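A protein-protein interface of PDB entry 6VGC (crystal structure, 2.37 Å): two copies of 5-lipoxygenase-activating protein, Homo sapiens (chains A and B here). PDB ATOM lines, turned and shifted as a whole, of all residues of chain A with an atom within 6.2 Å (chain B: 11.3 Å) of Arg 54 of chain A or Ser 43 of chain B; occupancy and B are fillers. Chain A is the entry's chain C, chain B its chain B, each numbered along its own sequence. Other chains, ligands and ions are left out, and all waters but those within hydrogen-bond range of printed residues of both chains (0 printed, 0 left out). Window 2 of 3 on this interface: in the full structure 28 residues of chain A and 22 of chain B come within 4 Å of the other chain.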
ATOM      1  N   THR A  49     -27.025 -12.860 -29.538  1.00  0.00           N
ATOM      2  CA  THR A  49     -28.106 -11.873 -29.598  1.00  0.00           C
ATOM      3  C   THR A  49     -27.693 -10.582 -28.887  1.00  0.00           C
ATOM      4  O   THR A  49     -26.912 -10.614 -27.932  1.00  0.00           O
ATOM      5  CB  THR A  49     -29.412 -12.424 -28.967  1.00  0.00           C
ATOM      6  OG1 THR A  49     -29.605 -13.787 -29.364  1.00  0.00           O
ATOM      7  CG2 THR A  49     -30.624 -11.608 -29.404  1.00  0.00           C
ATOM      8  N   LEU A  50     -28.212  -9.452 -29.367  1.00  0.00           N
ATOM      9  CA  LEU A  50     -27.954  -8.142 -28.761  1.00  0.00           C
ATOM     10  C   LEU A  50     -28.237  -8.149 -27.255  1.00  0.00           C
ATOM     11  O   LEU A  50     -27.496  -7.545 -26.479  1.00  0.00           O
ATOM     12  CB  LEU A  50     -28.773  -7.051 -29.471  1.00  0.00           C
ATOM     13  CG  LEU A  50     -28.483  -5.548 -29.292  1.00  0.00           C
ATOM     14  CD1 LEU A  50     -29.150  -4.966 -28.040  1.00  0.00           C
ATOM     15  CD2 LEU A  50     -26.982  -5.215 -29.326  1.00  0.00           C
ATOM     16  N   ALA A  51     -29.300  -8.846 -26.858  1.00  0.00           N
ATOM     17  CA  ALA A  51     -29.658  -9.006 -25.448  1.00  0.00           C
ATOM     18  C   ALA A  51     -28.590  -9.771 -24.662  1.00  0.00           C
ATOM     19  O   ALA A  51     -28.291  -9.425 -23.520  1.00  0.00           O
ATOM     20  CB  ALA A  51     -31.013  -9.690 -25.315  1.00  0.00           C
ATOM     21  N   PHE A  52     -28.022 -10.806 -25.280  1.00  0.00           N
ATOM     22  CA  PHE A  52     -26.974 -11.599 -24.644  1.00  0.00           C
ATOM     23  C   PHE A  52     -25.690 -10.798 -24.439  1.00  0.00           C
ATOM     24  O   PHE A  52     -25.107 -10.824 -23.356  1.00  0.00           O
ATOM     25  CB  PHE A  52     -26.691 -12.883 -25.435  1.00  0.00           C
ATOM     26  CG  PHE A  52     -25.463 -13.620 -24.973  1.00  0.00           C
ATOM     27  CD1 PHE A  52     -25.447 -14.276 -23.744  1.00  0.00           C
ATOM     28  CD2 PHE A  52     -24.318 -13.650 -25.765  1.00  0.00           C
ATOM     29  CE1 PHE A  52     -24.308 -14.954 -23.309  1.00  0.00           C
ATOM     30  CE2 PHE A  52     -23.175 -14.325 -25.339  1.00  0.00           C
ATOM     31  CZ  PHE A  52     -23.171 -14.978 -24.110  1.00  0.00           C
ATOM     32  N   GLU A  53     -25.262 -10.086 -25.482  1.00  0.00           N
ATOM     33  CA  GLU A  53     -24.021  -9.313 -25.437  1.00  0.00           C
ATOM     34  C   GLU A  53     -24.057  -8.203 -24.391  1.00  0.00           C
ATOM     35  O   GLU A  53     -23.027  -7.868 -23.807  1.00  0.00           O
ATOM     36  CB  GLU A  53     -23.680  -8.743 -26.816  1.00  0.00           C
ATOM     37  CG  GLU A  53     -23.150  -9.786 -27.794  1.00  0.00           C
ATOM     38  CD  GLU A  53     -22.660  -9.191 -29.104  1.00  0.00           C
ATOM     39  OE1 GLU A  53     -22.273  -8.001 -29.127  1.00  0.00           O
ATOM     40  OE2 GLU A  53     -22.652  -9.924 -30.115  1.00  0.00           O
ATOM     41  N   ARG A  54     -25.245  -7.648 -24.159  1.00  0.00           N
ATOM     42  CA  ARG A  54     -25.445  -6.626 -23.133  1.00  0.00           C
ATOM     43  C   ARG A  54     -25.230  -7.184 -21.725  1.00  0.00           C
ATOM     44  O   ARG A  54     -24.538  -6.571 -20.909  1.00  0.00           O
ATOM     45  CB  ARG A  54     -26.843  -6.007 -23.253  1.00  0.00           C
ATOM     46  CG  ARG A  54     -27.021  -5.048 -24.427  1.00  0.00           C
ATOM     47  CD  ARG A  54     -26.405  -3.686 -24.142  1.00  0.00           C
ATOM     48  NE  ARG A  54     -26.661  -2.729 -25.219  1.00  0.00           N
ATOM     49  CZ  ARG A  54     -27.745  -1.960 -25.308  1.00  0.00           C
ATOM     50  NH1 ARG A  54     -28.700  -2.027 -24.388  1.00  0.00           N
ATOM     51  NH2 ARG A  54     -27.876  -1.123 -26.327  1.00  0.00           N
ATOM     52  N   VAL A  55     -25.821  -8.348 -21.456  1.00  0.00           N
ATOM     53  CA  VAL A  55     -25.693  -9.023 -20.164  1.00  0.00           C
ATOM     54  C   VAL A  55     -24.258  -9.505 -19.942  1.00  0.00           C
ATOM     55  O   VAL A  55     -23.682  -9.281 -18.874  1.00  0.00           O
ATOM     56  CB  VAL A  55     -26.675 -10.221 -20.030  1.00  0.00           C
ATOM     57  CG1 VAL A  55     -26.614 -10.816 -18.627  1.00  0.00           C
ATOM     58  CG2 VAL A  55     -28.098  -9.788 -20.344  1.00  0.00           C
ATOM     59  N   TYR A  56     -23.693 -10.157 -20.959  1.00  0.00           N
ATOM     60  CA  TYR A  56     -22.324 -10.664 -20.901  1.00  0.00           C
ATOM     61  C   TYR A  56     -21.330  -9.547 -20.581  1.00  0.00           C
ATOM     62  O   TYR A  56     -20.481  -9.703 -19.701  1.00  0.00           O
ATOM     63  CB  TYR A  56     -21.943 -11.374 -22.206  1.00  0.00           C
ATOM     64  CG  TYR A  56     -20.564 -12.004 -22.179  1.00  0.00           C
ATOM     65  CD1 TYR A  56     -19.431 -11.272 -22.545  1.00  0.00           C
ATOM     66  CD2 TYR A  56     -20.390 -13.332 -21.783  1.00  0.00           C
ATOM     67  CE1 TYR A  56     -18.163 -11.843 -22.514  1.00  0.00           C
ATOM     68  CE2 TYR A  56     -19.123 -13.913 -21.752  1.00  0.00           C
ATOM     69  CZ  TYR A  56     -18.016 -13.162 -22.119  1.00  0.00           C
ATOM     70  OH  TYR A  56     -16.763 -13.727 -22.091  1.00  0.00           O
ATOM     71  N   THR A  57     -21.452  -8.425 -21.290  1.00  0.00           N
ATOM     72  CA  THR A  57     -20.596  -7.257 -21.068  1.00  0.00           C
ATOM     73  C   THR A  57     -20.745  -6.722 -19.643  1.00  0.00           C
ATOM     74  O   THR A  57     -19.745  -6.483 -18.960  1.00  0.00           O
ATOM     75  CB  THR A  57     -20.881  -6.137 -22.102  1.00  0.00           C
ATOM     76  OG1 THR A  57     -20.733  -6.659 -23.427  1.00  0.00           O
ATOM     77  CG2 THR A  57     -19.921  -4.970 -21.929  1.00  0.00           C
ATOM     78  N   ALA A  58     -21.990  -6.556 -19.200  1.00  0.00           N
ATOM     79  CA  ALA A  58     -22.298  -6.046 -17.859  1.00  0.00           C
ATOM     80  C   ALA A  58     -21.674  -6.912 -16.773  1.00  0.00           C
ATOM     81  O   ALA A  58     -21.064  -6.399 -15.833  1.00  0.00           O
ATOM     82  CB  ALA A  58     -23.801  -5.958 -17.659  1.00  0.00           C
ATOM     83  N   ASN A  59     -21.846  -8.224 -16.912  1.00  0.00           N
ATOM     84  CA  ASN A  59     -21.244  -9.204 -16.018  1.00  0.00           C
ATOM     85  C   ASN A  59     -19.722  -9.106 -16.014  1.00  0.00           C
ATOM     86  O   ASN A  59     -19.101  -9.082 -14.950  1.00  0.00           O
ATOM     87  CB  ASN A  59     -21.683 -10.616 -16.417  1.00  0.00           C
ATOM     88  CG  ASN A  59     -21.058 -11.695 -15.553  1.00  0.00           C
ATOM     89  OD1 ASN A  59     -20.356 -12.578 -16.053  1.00  0.00           O
ATOM     90  ND2 ASN A  59     -21.308 -11.628 -14.252  1.00  0.00           N
ATOM     91  N   GLY A 102     -29.003  -1.461 -15.297  1.00  0.00           N
ATOM     92  CA  GLY A 102     -28.924  -0.421 -16.326  1.00  0.00           C
ATOM     93  C   GLY A 102     -28.597  -0.946 -17.714  1.00  0.00           C
ATOM     94  O   GLY A 102     -29.047  -0.386 -18.715  1.00  0.00           O
ATOM     95  N   TYR A 103     -27.813  -2.021 -17.770  1.00  0.00           N
ATOM     96  CA  TYR A 103     -27.467  -2.681 -19.030  1.00  0.00           C
ATOM     97  C   TYR A 103     -28.621  -3.500 -19.602  1.00  0.00           C
ATOM     98  O   TYR A 103     -28.661  -3.768 -20.805  1.00  0.00           O
ATOM     99  CB  TYR A 103     -26.241  -3.580 -18.846  1.00  0.00           C
ATOM    100  CG  TYR A 103     -24.916  -2.871 -19.021  1.00  0.00           C
ATOM    101  CD1 TYR A 103     -24.382  -2.087 -18.002  1.00  0.00           C
ATOM    102  CD2 TYR A 103     -24.191  -2.993 -20.206  1.00  0.00           C
ATOM    103  CE1 TYR A 103     -23.167  -1.436 -18.159  1.00  0.00           C
ATOM    104  CE2 TYR A 103     -22.973  -2.345 -20.373  1.00  0.00           C
ATOM    105  CZ  TYR A 103     -22.467  -1.569 -19.345  1.00  0.00           C
ATOM    106  OH  TYR A 103     -21.262  -0.924 -19.500  1.00  0.00           O
ATOM    107  N   LEU A 104     -29.557  -3.889 -18.739  1.00  0.00           N
ATOM    108  CA  LEU A 104     -30.693  -4.725 -19.132  1.00  0.00           C
ATOM    109  C   LEU A 104     -31.813  -3.938 -19.829  1.00  0.00           C
ATOM    110  O   LEU A 104     -32.912  -4.463 -20.037  1.00  0.00           O
ATOM    111  CB  LEU A 104     -31.247  -5.482 -17.915  1.00  0.00           C
ATOM    112  CG  LEU A 104     -30.326  -6.429 -17.133  1.00  0.00           C
ATOM    113  CD1 LEU A 104     -30.957  -6.807 -15.798  1.00  0.00           C
ATOM    114  CD2 LEU A 104     -29.988  -7.677 -17.935  1.00  0.00           C
ATOM    115  N   GLY A 105     -31.527  -2.688 -20.192  1.00  0.00           N
ATOM    116  CA  GLY A 105     -32.496  -1.825 -20.867  1.00  0.00           C
ATOM    117  C   GLY A 105     -32.779  -2.250 -22.296  1.00  0.00           C
ATOM    118  O   GLY A 105     -32.445  -1.539 -23.245  1.00  0.00           O
ATOM    119  N   THR A 111     -26.806   2.341 -22.044  1.00  0.00           N
ATOM    120  CA  THR A 111     -26.209   1.696 -20.878  1.00  0.00           C
ATOM    121  C   THR A 111     -25.149   2.597 -20.231  1.00  0.00           C
ATOM    122  O   THR A 111     -24.559   3.440 -20.915  1.00  0.00           O
ATOM    123  CB  THR A 111     -25.570   0.325 -21.239  1.00  0.00           C
ATOM    124  OG1 THR A 111     -24.396   0.525 -22.036  1.00  0.00           O
ATOM    125  CG2 THR A 111     -26.559  -0.560 -21.995  1.00  0.00           C
ATOM    126  N   PRO A 112     -24.910   2.428 -18.911  1.00  0.00           N
ATOM    127  CA  PRO A 112     -23.825   3.136 -18.220  1.00  0.00           C
ATOM    128  C   PRO A 112     -22.442   2.780 -18.773  1.00  0.00           C
ATOM    129  O   PRO A 112     -22.315   1.854 -19.576  1.00  0.00           O
ATOM    130  CB  PRO A 112     -23.950   2.642 -16.774  1.00  0.00           C
ATOM    131  CG  PRO A 112     -25.364   2.221 -16.637  1.00  0.00           C
ATOM    132  CD  PRO A 112     -25.738   1.653 -17.968  1.00  0.00           C
ATOM    133  N   VAL B  32      -9.547   2.381 -20.028  1.00  0.00           N
ATOM    134  CA  VAL B  32     -10.631   1.751 -20.780  1.00  0.00           C
ATOM    135  C   VAL B  32     -11.829   2.701 -20.873  1.00  0.00           C
ATOM    136  O   VAL B  32     -12.451   2.819 -21.929  1.00  0.00           O
ATOM    137  CB  VAL B  32     -11.041   0.382 -20.163  1.00  0.00           C
ATOM    138  CG1 VAL B  32     -12.253  -0.215 -20.878  1.00  0.00           C
ATOM    139  CG2 VAL B  32      -9.872  -0.593 -20.214  1.00  0.00           C
ATOM    140  N   GLU B  33     -12.129   3.381 -19.766  1.00  0.00           N
ATOM    141  CA  GLU B  33     -13.227   4.348 -19.695  1.00  0.00           C
ATOM    142  C   GLU B  33     -13.047   5.494 -20.693  1.00  0.00           C
ATOM    143  O   GLU B  33     -13.987   5.863 -21.399  1.00  0.00           O
ATOM    144  CB  GLU B  33     -13.347   4.905 -18.271  1.00  0.00           C
ATOM    145  CG  GLU B  33     -14.505   5.879 -18.043  1.00  0.00           C
ATOM    146  CD  GLU B  33     -15.793   5.199 -17.608  1.00  0.00           C
ATOM    147  OE1 GLU B  33     -16.159   4.152 -18.186  1.00  0.00           O
ATOM    148  OE2 GLU B  33     -16.451   5.721 -16.684  1.00  0.00           O
ATOM    149  N   GLU B  35     -11.203   5.657 -23.502  1.00  0.00           N
ATOM    150  CA  GLU B  35     -11.263   5.224 -24.896  1.00  0.00           C
ATOM    151  C   GLU B  35     -12.661   4.748 -25.305  1.00  0.00           C
ATOM    152  O   GLU B  35     -12.988   4.718 -26.492  1.00  0.00           O
ATOM    153  CB  GLU B  35     -10.212   4.142 -25.164  1.00  0.00           C
ATOM    154  CG  GLU B  35      -9.760   4.035 -26.621  1.00  0.00           C
ATOM    155  CD  GLU B  35      -8.938   5.228 -27.099  1.00  0.00           C
ATOM    156  OE1 GLU B  35      -8.231   5.855 -26.279  1.00  0.00           O
ATOM    157  OE2 GLU B  35      -8.992   5.533 -28.309  1.00  0.00           O
ATOM    158  N   SER B  36     -13.481   4.389 -24.318  1.00  0.00           N
ATOM    159  CA  SER B  36     -14.856   3.953 -24.568  1.00  0.00           C
ATOM    160  C   SER B  36     -15.802   5.121 -24.846  1.00  0.00           C
ATOM    161  O   SER B  36     -16.898   4.927 -25.375  1.00  0.00           O
ATOM    162  CB  SER B  36     -15.385   3.121 -23.396  1.00  0.00           C
ATOM    163  OG  SER B  36     -15.551   3.909 -22.230  1.00  0.00           O
ATOM    164  N   ARG B  37     -15.373   6.328 -24.482  1.00  0.00           N
ATOM    165  CA  ARG B  37     -16.175   7.536 -24.685  1.00  0.00           C
ATOM    166  C   ARG B  37     -15.940   8.177 -26.055  1.00  0.00           C
ATOM    167  O   ARG B  37     -16.646   9.115 -26.437  1.00  0.00           O
ATOM    168  CB  ARG B  37     -15.933   8.540 -23.553  1.00  0.00           C
ATOM    169  CG  ARG B  37     -16.613   8.154 -22.248  1.00  0.00           C
ATOM    170  CD  ARG B  37     -16.157   9.022 -21.089  1.00  0.00           C
ATOM    171  NE  ARG B  37     -16.837   8.655 -19.847  1.00  0.00           N
ATOM    172  CZ  ARG B  37     -16.532   9.135 -18.644  1.00  0.00           C
ATOM    173  NH1 ARG B  37     -15.546  10.012 -18.496  1.00  0.00           N
ATOM    174  NH2 ARG B  37     -17.216   8.734 -17.581  1.00  0.00           N
ATOM    175  N   THR B  38     -14.950   7.665 -26.786  1.00  0.00           N
ATOM    176  CA  THR B  38     -14.692   8.083 -28.165  1.00  0.00           C
ATOM    177  C   THR B  38     -15.498   7.233 -29.151  1.00  0.00           C
ATOM    178  O   THR B  38     -15.528   7.518 -30.352  1.00  0.00           O
ATOM    179  CB  THR B  38     -13.187   8.005 -28.528  1.00  0.00           C
ATOM    180  OG1 THR B  38     -12.720   6.658 -28.377  1.00  0.00           O
ATOM    181  CG2 THR B  38     -12.361   8.931 -27.643  1.00  0.00           C
ATOM    182  N   GLN B  39     -16.151   6.194 -28.631  1.00  0.00           N
ATOM    183  CA  GLN B  39     -16.937   5.263 -29.441  1.00  0.00           C
ATOM    184  C   GLN B  39     -18.258   5.890 -29.874  1.00  0.00           C
ATOM    185  O   GLN B  39     -18.336   6.543 -30.915  1.00  0.00           O
ATOM    186  CB  GLN B  39     -17.201   3.961 -28.674  1.00  0.00           C
ATOM    187  CG  GLN B  39     -15.953   3.267 -28.118  1.00  0.00           C
ATOM    188  CD  GLN B  39     -15.046   2.700 -29.198  1.00  0.00           C
ATOM    189  OE1 GLN B  39     -14.000   3.273 -29.506  1.00  0.00           O
ATOM    190  NE2 GLN B  39     -15.442   1.572 -29.775  1.00  0.00           N
ATOM    191  N   SER B  43     -23.965   3.379 -25.354  1.00  0.00           N
ATOM    192  CA  SER B  43     -23.908   1.951 -25.053  1.00  0.00           C
ATOM    193  C   SER B  43     -22.473   1.421 -25.091  1.00  0.00           C
ATOM    194  O   SER B  43     -21.735   1.671 -26.048  1.00  0.00           O
ATOM    195  CB  SER B  43     -24.791   1.161 -26.022  1.00  0.00           C
ATOM    196  N   PHE B  44     -22.092   0.696 -24.042  1.00  0.00           N
ATOM    197  CA  PHE B  44     -20.756   0.104 -23.939  1.00  0.00           C
ATOM    198  C   PHE B  44     -20.743  -1.335 -24.461  1.00  0.00           C
ATOM    199  O   PHE B  44     -21.598  -2.148 -24.099  1.00  0.00           O
ATOM    200  CB  PHE B  44     -20.247   0.166 -22.490  1.00  0.00           C
ATOM    201  CG  PHE B  44     -18.849  -0.372 -22.307  1.00  0.00           C
ATOM    202  CD1 PHE B  44     -18.637  -1.722 -22.038  1.00  0.00           C
ATOM    203  CD2 PHE B  44     -17.747   0.470 -22.395  1.00  0.00           C
ATOM    204  CE1 PHE B  44     -17.352  -2.229 -21.872  1.00  0.00           C
ATOM    205  CE2 PHE B  44     -16.454  -0.028 -22.226  1.00  0.00           C
ATOM    206  CZ  PHE B  44     -16.259  -1.380 -21.964  1.00  0.00           C
ATOM    207  N   GLN B  45     -19.763  -1.629 -25.311  1.00  0.00           N
ATOM    208  CA  GLN B  45     -19.588  -2.956 -25.895  1.00  0.00           C
ATOM    209  C   GLN B  45     -18.116  -3.370 -25.842  1.00  0.00           C
ATOM    210  O   GLN B  45     -17.255  -2.565 -25.481  1.00  0.00           O
ATOM    211  CB  GLN B  45     -20.096  -2.973 -27.338  1.00  0.00           C
ATOM    212  N   ARG B  46     -17.835  -4.620 -26.199  1.00  0.00           N
ATOM    213  CA  ARG B  46     -16.466  -5.146 -26.183  1.00  0.00           C
ATOM    214  C   ARG B  46     -15.721  -4.937 -27.504  1.00  0.00           C
ATOM    215  O   ARG B  46     -14.490  -4.848 -27.520  1.00  0.00           O
ATOM    216  CB  ARG B  46     -16.462  -6.628 -25.800  1.00  0.00           C
ATOM    217  CG  ARG B  46     -16.855  -6.897 -24.350  1.00  0.00           C
ATOM    218  CD  ARG B  46     -16.752  -8.375 -23.990  1.00  0.00           C
ATOM    219  NE  ARG B  46     -17.741  -9.191 -24.691  1.00  0.00           N
ATOM    220  CZ  ARG B  46     -17.470  -9.997 -25.714  1.00  0.00           C
ATOM    221  NH1 ARG B  46     -16.228 -10.114 -26.172  1.00  0.00           N
ATOM    222  NH2 ARG B  46     -18.446 -10.693 -26.281  1.00  0.00           N
ATOM    223  N   THR B  47     -16.469  -4.861 -28.603  1.00  0.00           N
ATOM    224  CA  THR B  47     -15.893  -4.706 -29.939  1.00  0.00           C
ATOM    225  C   THR B  47     -16.194  -3.331 -30.538  1.00  0.00           C
ATOM    226  O   THR B  47     -17.332  -2.854 -30.477  1.00  0.00           O
ATOM    227  CB  THR B  47     -16.391  -5.809 -30.900  1.00  0.00           C
ATOM    228  N   GLY B  48     -15.170  -2.703 -31.113  1.00  0.00           N
ATOM    229  CA  GLY B  48     -15.309  -1.383 -31.730  1.00  0.00           C
ATOM    230  C   GLY B  48     -14.071  -0.944 -32.490  1.00  0.00           C
ATOM    231  O   GLY B  48     -13.614  -1.632 -33.405  1.00  0.00           O
ATOM    232  N   THR B  49     -13.531   0.210 -32.104  1.00  0.00           N
ATOM    233  CA  THR B  49     -12.322   0.761 -32.717  1.00  0.00           C
ATOM    234  C   THR B  49     -11.110  -0.103 -32.363  1.00  0.00           C
ATOM    235  O   THR B  49     -11.085  -0.739 -31.307  1.00  0.00           O
ATOM    236  CB  THR B  49     -12.076   2.221 -32.259  1.00  0.00           C
ATOM    237  OG1 THR B  49     -13.316   2.939 -32.253  1.00  0.00           O
ATOM    238  CG2 THR B  49     -11.097   2.933 -33.187  1.00  0.00           C
ATOM    239  N   PHE B  52      -9.696   1.126 -29.081  1.00  0.00           N
ATOM    240  CA  PHE B  52     -10.451   0.679 -27.909  1.00  0.00           C
ATOM    241  C   PHE B  52     -10.243  -0.804 -27.606  1.00  0.00           C
ATOM    242  O   PHE B  52     -10.043  -1.178 -26.449  1.00  0.00           O
ATOM    243  CB  PHE B  52     -11.948   0.988 -28.054  1.00  0.00           C
ATOM    244  CG  PHE B  52     -12.806   0.322 -27.011  1.00  0.00           C
ATOM    245  CD1 PHE B  52     -12.850   0.811 -25.708  1.00  0.00           C
ATOM    246  CD2 PHE B  52     -13.557  -0.808 -27.326  1.00  0.00           C
ATOM    247  CE1 PHE B  52     -13.633   0.191 -24.739  1.00  0.00           C
ATOM    248  CE2 PHE B  52     -14.342  -1.434 -26.362  1.00  0.00           C
ATOM    249  CZ  PHE B  52     -14.380  -0.933 -25.067  1.00  0.00           C
ATOM    250  N   TYR B  56      -8.802  -2.460 -24.187  1.00  0.00           N
ATOM    251  CA  TYR B  56      -9.724  -3.348 -23.478  1.00  0.00           C
ATOM    252  C   TYR B  56      -9.125  -4.741 -23.268  1.00  0.00           C
ATOM    253  O   TYR B  56      -9.255  -5.317 -22.189  1.00  0.00           O
ATOM    254  CB  TYR B  56     -11.071  -3.446 -24.211  1.00  0.00           C
ATOM    255  CG  TYR B  56     -12.094  -4.296 -23.487  1.00  0.00           C
ATOM    256  CD1 TYR B  56     -12.180  -5.673 -23.722  1.00  0.00           C
ATOM    257  CD2 TYR B  56     -12.969  -3.729 -22.557  1.00  0.00           C
ATOM    258  CE1 TYR B  56     -13.107  -6.459 -23.050  1.00  0.00           C
ATOM    259  CE2 TYR B  56     -13.903  -4.510 -21.881  1.00  0.00           C
ATOM    260  CZ  TYR B  56     -13.965  -5.873 -22.134  1.00  0.00           C
ATOM    261  OH  TYR B  56     -14.885  -6.651 -21.473  1.00  0.00           O
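Among the printed residues, merely in contact across the chains: Arg 54 of chain A with Ser 43 of chain B (3.9 Å), Tyr 56 of chain A with Arg 46 of chain B (3.4 Å), Thr 57 of chain A with Phe 44 of chain B (3.5 Å), Thr 57 of chain A with Arg 46 of chain B (3.99 Å), Tyr 103 of chain A with Phe 44 of chain B (3.3 Å), Thr 111 of chain A with Ser 43 of chain B (3.4 Å) and Pro 112 of chain A with Phe 44 of chain B (3.95 Å).
Of the 17 printed residues of chain A, 6 touch a printed residue of chain B. Printed residues of chain A that touch a printed residue of chain B: Arg 54, Tyr 56, Thr 57, Tyr 103, Thr 111 and Pro 112. Hydrophobic or aromatic side chains of chain A within 4 Å of the printed part of chain B: Tyr 56 and Tyr 103. Among the printed residues, no Asp or Glu carboxylate lies within 4 Å of a Lys or Arg side-chain nitrogen of the other chain.
The side-chain hydroxyl (OG1) of Thr 111 of chain A lies within hydrogen-bond range of the backbone NH (N) of Phe 44 of chain B, 3.1 Å away.
OH of Tyr 103 of chain A lies within hydrogen-bond range of O of Pro 112 of chain A (3.0 Å). The backbone carbonyl oxygen of Glu 53 of chain A is in hydrogen-bond range of the side-chain hydroxyl of Thr 57 of chain A (2.6 Å).
Arg 54 of chain A touches just one residue of chain B: Ser 43. Of chain A, only Arg 54 and Thr 111 come within 4 Å of Ser 43 of chain B. No residue of chain B comes within 4 Å of Leu 50 of chain A. No residue of chain B comes within 4 Å of Ala 51 of chain A. No residue of chain B comes within 4 Å of Glu 53 of chain A. No residue of chain B comes within 4 Å of Val 55 of chain A. Ala 58 of chain A touches none of the printed residues of chain B. Gly 105 of chain A touches none of the printed residues of chain B. Of the printed residues of chain A, Phe 44 of chain B touches Thr 57, Tyr 103, Thr 111 and Pro 112. Printed residues of chain A within 4 Å of Arg 46 of chain B: Tyr 56 and Thr 57. Thr 47 of chain B touches none of the printed residues of chain A. The nearest printed residue of chain B that does not touch Tyr 56 of chain A is Tyr 56 of chain B (6.2 Å).
Positions printed for both chains: 49, 52 and 56.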
